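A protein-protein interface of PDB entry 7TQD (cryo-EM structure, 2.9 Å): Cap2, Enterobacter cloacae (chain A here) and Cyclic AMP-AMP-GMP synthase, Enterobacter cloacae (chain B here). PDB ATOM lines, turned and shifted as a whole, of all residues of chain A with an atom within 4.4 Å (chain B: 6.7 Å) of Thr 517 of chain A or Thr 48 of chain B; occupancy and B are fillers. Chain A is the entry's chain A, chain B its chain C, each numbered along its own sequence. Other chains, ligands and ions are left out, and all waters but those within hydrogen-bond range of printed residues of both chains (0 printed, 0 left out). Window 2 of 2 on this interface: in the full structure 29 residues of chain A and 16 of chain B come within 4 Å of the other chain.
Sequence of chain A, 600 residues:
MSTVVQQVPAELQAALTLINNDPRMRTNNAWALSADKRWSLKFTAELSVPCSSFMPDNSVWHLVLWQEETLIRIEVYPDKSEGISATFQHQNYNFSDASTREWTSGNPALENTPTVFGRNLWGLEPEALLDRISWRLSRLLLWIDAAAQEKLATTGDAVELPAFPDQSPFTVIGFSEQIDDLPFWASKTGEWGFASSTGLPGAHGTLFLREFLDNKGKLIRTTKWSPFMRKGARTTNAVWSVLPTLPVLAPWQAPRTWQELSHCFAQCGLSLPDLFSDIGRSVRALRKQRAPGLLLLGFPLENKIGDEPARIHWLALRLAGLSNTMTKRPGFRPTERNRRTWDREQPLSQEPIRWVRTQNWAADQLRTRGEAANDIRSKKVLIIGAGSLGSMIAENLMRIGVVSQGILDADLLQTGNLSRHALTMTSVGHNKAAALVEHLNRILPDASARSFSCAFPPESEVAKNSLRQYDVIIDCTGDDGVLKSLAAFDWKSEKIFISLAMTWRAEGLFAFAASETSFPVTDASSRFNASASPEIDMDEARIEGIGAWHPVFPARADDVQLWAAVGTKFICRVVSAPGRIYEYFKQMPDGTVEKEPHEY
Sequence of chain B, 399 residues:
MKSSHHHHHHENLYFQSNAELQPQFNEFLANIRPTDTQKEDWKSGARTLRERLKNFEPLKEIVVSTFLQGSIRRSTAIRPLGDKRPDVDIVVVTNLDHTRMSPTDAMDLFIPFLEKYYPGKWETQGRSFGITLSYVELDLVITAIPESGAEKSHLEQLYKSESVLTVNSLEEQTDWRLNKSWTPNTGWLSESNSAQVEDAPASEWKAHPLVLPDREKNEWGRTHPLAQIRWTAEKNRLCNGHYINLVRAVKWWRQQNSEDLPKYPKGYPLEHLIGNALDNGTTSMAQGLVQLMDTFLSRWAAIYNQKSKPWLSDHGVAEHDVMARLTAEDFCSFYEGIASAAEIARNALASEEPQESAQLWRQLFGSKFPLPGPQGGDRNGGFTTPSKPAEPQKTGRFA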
ATOM      1  N   TRP A 491       4.054  -6.639  -2.482  1.00  0.00           N
ATOM      2  CA  TRP A 491       3.736  -7.881  -3.173  1.00  0.00           C
ATOM      3  C   TRP A 491       2.448  -7.808  -3.979  1.00  0.00           C
ATOM      4  O   TRP A 491       2.245  -8.643  -4.867  1.00  0.00           O
ATOM      5  CB  TRP A 491       3.643  -9.029  -2.165  1.00  0.00           C
ATOM      6  CG  TRP A 491       4.921  -9.267  -1.423  1.00  0.00           C
ATOM      7  CD1 TRP A 491       5.250  -8.789  -0.190  1.00  0.00           C
ATOM      8  CD2 TRP A 491       6.044 -10.033  -1.868  1.00  0.00           C
ATOM      9  NE1 TRP A 491       6.506  -9.214   0.162  1.00  0.00           N
ATOM     10  CE2 TRP A 491       7.015  -9.978  -0.852  1.00  0.00           C
ATOM     11  CE3 TRP A 491       6.323 -10.760  -3.029  1.00  0.00           C
ATOM     12  CZ2 TRP A 491       8.241 -10.624  -0.960  1.00  0.00           C
ATOM     13  CZ3 TRP A 491       7.542 -11.398  -3.132  1.00  0.00           C
ATOM     14  CH2 TRP A 491       8.485 -11.326  -2.104  1.00  0.00           C
ATOM     15  N   SER A 493      -0.537  -8.634  -3.510  1.00  0.00           N
ATOM     16  CA  SER A 493      -1.549  -9.668  -3.340  1.00  0.00           C
ATOM     17  C   SER A 493      -1.257 -10.424  -2.053  1.00  0.00           C
ATOM     18  O   SER A 493      -0.306 -10.117  -1.331  1.00  0.00           O
ATOM     19  CB  SER A 493      -1.598 -10.620  -4.539  1.00  0.00           C
ATOM     20  OG  SER A 493      -0.371 -11.301  -4.701  1.00  0.00           O
ATOM     21  N   GLU A 494      -2.092 -11.420  -1.774  1.00  0.00           N
ATOM     22  CA  GLU A 494      -1.965 -12.195  -0.548  1.00  0.00           C
ATOM     23  C   GLU A 494      -1.014 -13.366  -0.763  1.00  0.00           C
ATOM     24  O   GLU A 494      -1.124 -14.092  -1.755  1.00  0.00           O
ATOM     25  CB  GLU A 494      -3.333 -12.697  -0.090  1.00  0.00           C
ATOM     26  CG  GLU A 494      -3.365 -13.171   1.352  1.00  0.00           C
ATOM     27  CD  GLU A 494      -4.741 -13.629   1.787  1.00  0.00           C
ATOM     28  OE1 GLU A 494      -5.708 -13.419   1.024  1.00  0.00           O
ATOM     29  OE2 GLU A 494      -4.859 -14.193   2.893  1.00  0.00           O
ATOM     30  N   PHE A 497       3.786 -16.611   4.032  1.00  0.00           N
ATOM     31  CA  PHE A 497       5.160 -16.334   4.426  1.00  0.00           C
ATOM     32  C   PHE A 497       5.594 -17.310   5.510  1.00  0.00           C
ATOM     33  O   PHE A 497       4.920 -17.443   6.536  1.00  0.00           O
ATOM     34  CB  PHE A 497       5.300 -14.897   4.927  1.00  0.00           C
ATOM     35  CG  PHE A 497       4.953 -13.864   3.896  1.00  0.00           C
ATOM     36  CD1 PHE A 497       5.846 -13.541   2.889  1.00  0.00           C
ATOM     37  CD2 PHE A 497       3.731 -13.219   3.931  1.00  0.00           C
ATOM     38  CE1 PHE A 497       5.524 -12.596   1.941  1.00  0.00           C
ATOM     39  CE2 PHE A 497       3.407 -12.274   2.983  1.00  0.00           C
ATOM     40  CZ  PHE A 497       4.304 -11.963   1.988  1.00  0.00           C
ATOM     41  N   GLU A 516      -0.702 -13.169   4.745  1.00  0.00           N
ATOM     42  CA  GLU A 516      -1.119 -11.778   4.652  1.00  0.00           C
ATOM     43  C   GLU A 516      -0.655 -11.200   3.323  1.00  0.00           C
ATOM     44  O   GLU A 516      -0.105 -11.901   2.470  1.00  0.00           O
ATOM     45  CB  GLU A 516      -0.558 -10.943   5.810  1.00  0.00           C
ATOM     46  CG  GLU A 516      -1.108 -11.302   7.177  1.00  0.00           C
ATOM     47  CD  GLU A 516      -2.452 -10.665   7.449  1.00  0.00           C
ATOM     48  OE1 GLU A 516      -2.561  -9.429   7.327  1.00  0.00           O
ATOM     49  OE2 GLU A 516      -3.402 -11.401   7.792  1.00  0.00           O
ATOM     50  N   THR A 517      -0.896  -9.898   3.155  1.00  0.00           N
ATOM     51  CA  THR A 517      -0.332  -9.159   2.033  1.00  0.00           C
ATOM     52  C   THR A 517       1.062  -8.634   2.350  1.00  0.00           C
ATOM     53  O   THR A 517       1.883  -8.468   1.441  1.00  0.00           O
ATOM     54  CB  THR A 517      -1.254  -8.000   1.652  1.00  0.00           C
ATOM     55  OG1 THR A 517      -2.606  -8.466   1.593  1.00  0.00           O
ATOM     56  CG2 THR A 517      -0.869  -7.424   0.303  1.00  0.00           C
ATOM     57  N   SER A 518       1.347  -8.377   3.626  1.00  0.00           N
ATOM     58  CA  SER A 518       2.647  -7.907   4.072  1.00  0.00           C
ATOM     59  C   SER A 518       3.170  -8.826   5.165  1.00  0.00           C
ATOM     60  O   SER A 518       2.397  -9.404   5.933  1.00  0.00           O
ATOM     61  CB  SER A 518       2.575  -6.469   4.592  1.00  0.00           C
ATOM     62  OG  SER A 518       3.857  -5.998   4.972  1.00  0.00           O
ATOM     63  N   LYS B  43      -2.742  -2.545  10.407  1.00  0.00           N
ATOM     64  CA  LYS B  43      -2.390  -2.170   9.040  1.00  0.00           C
ATOM     65  C   LYS B  43      -2.508  -3.360   8.095  1.00  0.00           C
ATOM     66  O   LYS B  43      -3.160  -3.279   7.042  1.00  0.00           O
ATOM     67  CB  LYS B  43      -0.973  -1.599   9.001  1.00  0.00           C
ATOM     68  CG  LYS B  43      -0.837  -0.245   9.658  1.00  0.00           C
ATOM     69  CD  LYS B  43       0.517   0.365   9.374  1.00  0.00           C
ATOM     70  CE  LYS B  43       0.602   1.770   9.924  1.00  0.00           C
ATOM     71  NZ  LYS B  43       1.838   2.458   9.470  1.00  0.00           N
ATOM     72  N   SER B  44      -1.889  -4.486   8.465  1.00  0.00           N
ATOM     73  CA  SER B  44      -1.944  -5.669   7.616  1.00  0.00           C
ATOM     74  C   SER B  44      -3.364  -6.208   7.510  1.00  0.00           C
ATOM     75  O   SER B  44      -3.774  -6.679   6.443  1.00  0.00           O
ATOM     76  CB  SER B  44      -0.994  -6.740   8.149  1.00  0.00           C
ATOM     77  OG  SER B  44      -1.350  -7.125   9.463  1.00  0.00           O
ATOM     78  N   GLY B  45      -4.131  -6.144   8.599  1.00  0.00           N
ATOM     79  CA  GLY B  45      -5.508  -6.601   8.549  1.00  0.00           C
ATOM     80  C   GLY B  45      -6.364  -5.776   7.608  1.00  0.00           C
ATOM     81  O   GLY B  45      -7.153  -6.323   6.835  1.00  0.00           O
ATOM     82  N   ALA B  46      -6.218  -4.450   7.657  1.00  0.00           N
ATOM     83  CA  ALA B  46      -6.971  -3.592   6.752  1.00  0.00           C
ATOM     84  C   ALA B  46      -6.599  -3.866   5.301  1.00  0.00           C
ATOM     85  O   ALA B  46      -7.476  -3.975   4.433  1.00  0.00           O
ATOM     86  CB  ALA B  46      -6.736  -2.124   7.105  1.00  0.00           C
ATOM     87  N   ARG B  47      -5.299  -3.993   5.014  1.00  0.00           N
ATOM     88  CA  ARG B  47      -4.895  -4.261   3.635  1.00  0.00           C
ATOM     89  C   ARG B  47      -5.417  -5.611   3.152  1.00  0.00           C
ATOM     90  O   ARG B  47      -5.918  -5.726   2.022  1.00  0.00           O
ATOM     91  CB  ARG B  47      -3.378  -4.193   3.504  1.00  0.00           C
ATOM     92  CG  ARG B  47      -2.801  -2.813   3.725  1.00  0.00           C
ATOM     93  CD  ARG B  47      -1.291  -2.845   3.624  1.00  0.00           C
ATOM     94  NE  ARG B  47      -0.658  -1.867   4.498  1.00  0.00           N
ATOM     95  CZ  ARG B  47       0.629  -1.876   4.812  1.00  0.00           C
ATOM     96  NH1 ARG B  47       1.447  -2.807   4.349  1.00  0.00           N
ATOM     97  NH2 ARG B  47       1.111  -0.927   5.610  1.00  0.00           N
ATOM     98  N   THR B  48      -5.316  -6.643   3.994  1.00  0.00           N
ATOM     99  CA  THR B  48      -5.780  -7.970   3.601  1.00  0.00           C
ATOM    100  C   THR B  48      -7.287  -7.987   3.388  1.00  0.00           C
ATOM    101  O   THR B  48      -7.779  -8.596   2.432  1.00  0.00           O
ATOM    102  CB  THR B  48      -5.387  -8.997   4.659  1.00  0.00           C
ATOM    103  OG1 THR B  48      -4.039  -8.755   5.082  1.00  0.00           O
ATOM    104  CG2 THR B  48      -5.489 -10.399   4.096  1.00  0.00           C
ATOM    105  N   LEU B  49      -8.035  -7.324   4.271  1.00  0.00           N
ATOM    106  CA  LEU B  49      -9.483  -7.261   4.115  1.00  0.00           C
ATOM    107  C   LEU B  49      -9.860  -6.542   2.829  1.00  0.00           C
ATOM    108  O   LEU B  49     -10.778  -6.968   2.121  1.00  0.00           O
ATOM    109  CB  LEU B  49     -10.108  -6.570   5.324  1.00  0.00           C
ATOM    110  CG  LEU B  49     -11.611  -6.302   5.293  1.00  0.00           C
ATOM    111  CD1 LEU B  49     -12.389  -7.602   5.293  1.00  0.00           C
ATOM    112  CD2 LEU B  49     -12.005  -5.448   6.479  1.00  0.00           C
ATOM    113  N   ARG B  50      -9.157  -5.455   2.506  1.00  0.00           N
ATOM    114  CA  ARG B  50      -9.440  -4.740   1.266  1.00  0.00           C
ATOM    115  C   ARG B  50      -9.187  -5.622   0.048  1.00  0.00           C
ATOM    116  O   ARG B  50     -10.005  -5.666  -0.880  1.00  0.00           O
ATOM    117  CB  ARG B  50      -8.599  -3.469   1.201  1.00  0.00           C
ATOM    118  CG  ARG B  50      -8.853  -2.618  -0.023  1.00  0.00           C
ATOM    119  CD  ARG B  50      -7.848  -1.491  -0.089  1.00  0.00           C
ATOM    120  NE  ARG B  50      -7.866  -0.704   1.138  1.00  0.00           N
ATOM    121  CZ  ARG B  50      -6.927   0.167   1.479  1.00  0.00           C
ATOM    122  NH1 ARG B  50      -5.867   0.374   0.717  1.00  0.00           N
ATOM    123  NH2 ARG B  50      -7.051   0.840   2.618  1.00  0.00           N
ATOM    124  N   GLU B  51      -8.063  -6.342   0.037  1.00  0.00           N
ATOM    125  CA  GLU B  51      -7.764  -7.206  -1.105  1.00  0.00           C
ATOM    126  C   GLU B  51      -8.797  -8.322  -1.241  1.00  0.00           C
ATOM    127  O   GLU B  51      -9.274  -8.618  -2.347  1.00  0.00           O
ATOM    128  CB  GLU B  51      -6.358  -7.785  -0.971  1.00  0.00           C
ATOM    129  CG  GLU B  51      -5.992  -8.756  -2.079  1.00  0.00           C
ATOM    130  CD  GLU B  51      -5.680  -8.061  -3.389  1.00  0.00           C
ATOM    131  OE1 GLU B  51      -5.224  -6.900  -3.357  1.00  0.00           O
ATOM    132  OE2 GLU B  51      -5.893  -8.675  -4.455  1.00  0.00           O
ATOM    133  N   ARG B  52      -9.162  -8.946  -0.119  1.00  0.00           N
ATOM    134  CA  ARG B  52     -10.141 -10.029  -0.156  1.00  0.00           C
ATOM    135  C   ARG B  52     -11.500  -9.531  -0.624  1.00  0.00           C
ATOM    136  O   ARG B  52     -12.188 -10.212  -1.392  1.00  0.00           O
ATOM    137  CB  ARG B  52     -10.248 -10.676   1.223  1.00  0.00           C
ATOM    138  CG  ARG B  52      -8.996 -11.421   1.640  1.00  0.00           C
ATOM    139  CD  ARG B  52      -8.987 -11.709   3.128  1.00  0.00           C
ATOM    140  NE  ARG B  52      -8.064 -12.785   3.465  1.00  0.00           N
ATOM    141  CZ  ARG B  52      -7.817 -13.199   4.699  1.00  0.00           C
ATOM    142  NH1 ARG B  52      -8.403 -12.644   5.745  1.00  0.00           N
ATOM    143  NH2 ARG B  52      -6.954 -14.192   4.888  1.00  0.00           N
ATOM    144  N   LEU B  53     -11.908  -8.344  -0.168  1.00  0.00           N
ATOM    145  CA  LEU B  53     -13.166  -7.767  -0.629  1.00  0.00           C
ATOM    146  C   LEU B  53     -13.121  -7.474  -2.121  1.00  0.00           C
ATOM    147  O   LEU B  53     -14.117  -7.660  -2.828  1.00  0.00           O
ATOM    148  CB  LEU B  53     -13.473  -6.492   0.153  1.00  0.00           C
ATOM    149  CG  LEU B  53     -14.453  -6.625   1.314  1.00  0.00           C
ATOM    150  CD1 LEU B  53     -14.463  -5.352   2.133  1.00  0.00           C
ATOM    151  CD2 LEU B  53     -15.843  -6.947   0.803  1.00  0.00           C
ATOM    152  N   PHE B 113     -19.275 -13.899   2.660  1.00  0.00           N
ATOM    153  CA  PHE B 113     -17.875 -13.489   2.643  1.00  0.00           C
ATOM    154  C   PHE B 113     -17.225 -13.707   4.004  1.00  0.00           C
ATOM    155  O   PHE B 113     -16.119 -14.255   4.101  1.00  0.00           O
ATOM    156  CB  PHE B 113     -17.787 -12.022   2.213  1.00  0.00           C
ATOM    157  CG  PHE B 113     -16.414 -11.427   2.333  1.00  0.00           C
ATOM    158  CD1 PHE B 113     -15.510 -11.531   1.293  1.00  0.00           C
ATOM    159  CD2 PHE B 113     -16.037 -10.739   3.474  1.00  0.00           C
ATOM    160  CE1 PHE B 113     -14.255 -10.980   1.395  1.00  0.00           C
ATOM    161  CE2 PHE B 113     -14.780 -10.188   3.582  1.00  0.00           C
ATOM    162  CZ  PHE B 113     -13.888 -10.308   2.542  1.00  0.00           C
ATOM    163  N   TYR B 118     -13.392 -15.641   7.141  1.00  0.00           N
ATOM    164  CA  TYR B 118     -13.188 -15.487   8.582  1.00  0.00           C
ATOM    165  C   TYR B 118     -14.092 -16.456   9.327  1.00  0.00           C
ATOM    166  O   TYR B 118     -15.064 -16.042   9.973  1.00  0.00           O
ATOM    167  CB  TYR B 118     -13.455 -14.048   9.023  1.00  0.00           C
ATOM    168  CG  TYR B 118     -12.561 -13.037   8.357  1.00  0.00           C
ATOM    169  CD1 TYR B 118     -11.352 -12.674   8.927  1.00  0.00           C
ATOM    170  CD2 TYR B 118     -12.915 -12.458   7.149  1.00  0.00           C
ATOM    171  CE1 TYR B 118     -10.528 -11.755   8.318  1.00  0.00           C
ATOM    172  CE2 TYR B 118     -12.096 -11.539   6.532  1.00  0.00           C
ATOM    173  CZ  TYR B 118     -10.904 -11.193   7.122  1.00  0.00           C
ATOM    174  OH  TYR B 118     -10.080 -10.278   6.514  1.00  0.00           O
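Of the 13 printed residues of chain B, 5 touch a printed residue of chain A. Printed residues of chain B that touch a printed residue of chain A: Ser 44, Gly 45, Arg 47, Thr 48 and Arg 52. Printed residues of chain A that touch a printed residue of chain B: Glu 494, Glu 516, Thr 517 and Ser 518. Among the printed residues, 6 pairs touch across the chains. Among the printed residues, Asp or Glu carboxylates within 4 Å of a Lys or Arg side-chain nitrogen of the other chain: Glu 494 of chain A with Arg 52 of chain B (2.9 Å).
Printed residues of chain B within 4 Å of Glu 494 of chain A: Arg 52. Printed residues of chain B within 4 Å of Glu 516 of chain A: Ser 44, Gly 45 and Thr 48. Thr 517 of chain A touches one residue of chain B. Of the printed residues of chain B, Ser 518 of chain A touches Arg 47 (3.8 Å). Of the printed residues of chain A, Arg 47 of chain B touches Ser 518 (3.8 Å). Thr 48 of chain B touches just these residues of chain A: Glu 516 and Thr 517. Of the printed residues of chain A, Arg 52 of chain B touches Glu 494. The nearest residue of chain A that does not touch Thr 48 of chain B is Glu 494 of chain A (4.03 Å). The nearest printed residue of chain B that does not touch Glu 494 of chain A is Thr 48 of chain B (4.03 Å).
Among the printed residues, pairs that only touch across the chains: Glu 516 of chain A with Gly 45 of chain B (3.9 Å), Thr 517 of chain A with Thr 48 of chain B (3.8 Å) and Ser 518 of chain A with Arg 47 of chain B (3.8 Å).
The guanidinium group of Arg 52 of chain B sits at hydrogen-bond distance from the side-chain hydroxyl of Tyr 118 of chain B (3.0 Å). O of Ser 44 of chain B lies within hydrogen-bond range of OG1 of Thr 48 of chain B, 2.5 Å away.
The side-chain hydroxyl (OG) of Ser 44 of chain B lies close to the side-chain carboxylate (OE1) of Glu 516 of chain A (3.4 Å). The side-chain carboxylate (OE1) of Glu 516 of chain A sits at hydrogen-bond distance from the side-chain hydroxyl (OG1) of Thr 48 of chain B (2.8 Å). The side-chain carboxylate of Glu 494 of chain A is in salt-bridge range of the guanidinium group of Arg 52 of chain B, 2.9 Å away.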
